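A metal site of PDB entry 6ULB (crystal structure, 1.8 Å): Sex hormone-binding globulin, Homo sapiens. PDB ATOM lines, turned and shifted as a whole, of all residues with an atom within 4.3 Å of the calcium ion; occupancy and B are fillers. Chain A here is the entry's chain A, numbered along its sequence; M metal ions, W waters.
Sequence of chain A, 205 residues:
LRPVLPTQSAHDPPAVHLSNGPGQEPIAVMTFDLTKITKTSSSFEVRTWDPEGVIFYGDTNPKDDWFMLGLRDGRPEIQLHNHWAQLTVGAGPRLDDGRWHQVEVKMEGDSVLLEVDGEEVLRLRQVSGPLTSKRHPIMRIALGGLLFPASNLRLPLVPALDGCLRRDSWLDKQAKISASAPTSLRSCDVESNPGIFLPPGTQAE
Of the 4 residues printed, 3 come within 4 Å of the calcium ion. The nearest printed residue that does not touch the calcium ion is Leu 161 (4.2 Å).
The calcium ion is bound by the backbone carbonyl oxygen (O) of Ala 160, at 2.4 Å. O of Glu 52 binds the calcium ion (2.4 Å). The calcium ion is bound by water W1, 2.5 Å away. The side-chain carboxylate (OD2) of Asp 50 binds the calcium ion, 2.5 Å away. The calcium ion is bound by water W2, 2.5 Å away. OD1 of Asp 50 is bound to the calcium ion.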
ATOM      1  N   ASP A  50     -14.358   6.004  20.218  1.00  0.00           N
ATOM      2  CA  ASP A  50     -15.609   6.369  20.887  1.00  0.00           C
ATOM      3  C   ASP A  50     -15.322   6.788  22.327  1.00  0.00           C
ATOM      4  O   ASP A  50     -14.669   6.052  23.050  1.00  0.00           O
ATOM      5  CB  ASP A  50     -16.547   5.167  20.866  1.00  0.00           C
ATOM      6  CG  ASP A  50     -17.971   5.515  21.258  1.00  0.00           C
ATOM      7  OD1 ASP A  50     -18.227   6.644  21.726  1.00  0.00           O
ATOM      8  OD2 ASP A  50     -18.839   4.631  21.084  1.00  0.00           O
ATOM      9  N   GLU A  52     -17.481   7.207  24.877  1.00  0.00           N
ATOM     10  CA  GLU A  52     -18.476   6.878  25.893  1.00  0.00           C
ATOM     11  C   GLU A  52     -19.176   5.567  25.565  1.00  0.00           C
ATOM     12  O   GLU A  52     -19.599   5.350  24.431  1.00  0.00           O
ATOM     13  CB  GLU A  52     -19.508   8.017  26.023  1.00  0.00           C
ATOM     14  CG  GLU A  52     -20.505   7.813  27.167  1.00  0.00           C
ATOM     15  CD  GLU A  52     -21.361   9.025  27.437  1.00  0.00           C
ATOM     16  OE1 GLU A  52     -20.827  10.153  27.428  1.00  0.00           O
ATOM     17  OE2 GLU A  52     -22.589   8.850  27.631  1.00  0.00           O
ATOM     18  N   ALA A 160     -23.857   2.164  24.075  1.00  0.00           N
ATOM     19  CA  ALA A 160     -23.229   1.593  22.883  1.00  0.00           C
ATOM     20  C   ALA A 160     -21.803   2.110  22.757  1.00  0.00           C
ATOM     21  O   ALA A 160     -21.584   3.312  22.557  1.00  0.00           O
ATOM     22  CB  ALA A 160     -24.048   1.923  21.627  1.00  0.00           C
ATOM     23  N   LEU A 161     -20.831   1.216  22.866  1.00  0.00           N
ATOM     24  CA  LEU A 161     -19.428   1.572  22.667  1.00  0.00           C
ATOM     25  C   LEU A 161     -18.993   1.018  21.318  1.00  0.00           C
ATOM     26  O   LEU A 161     -18.929  -0.206  21.130  1.00  0.00           O
ATOM     27  CB  LEU A 161     -18.538   1.036  23.788  1.00  0.00           C
ATOM     28  CG  LEU A 161     -17.093   1.522  23.703  1.00  0.00           C
ATOM     29  CD1 LEU A 161     -16.997   3.034  23.910  1.00  0.00           C
ATOM     30  CD2 LEU A 161     -16.205   0.790  24.691  1.00  0.00           C
HETATM   31 CA    CA M   1     -20.769   5.538  22.330  1.00  0.00          CA
HETATM   32  O   HOH W   1     -20.704   7.984  22.084  1.00  0.00           O
HETATM   33  O   HOH W   2     -22.758   6.095  23.819  1.00  0.00           O
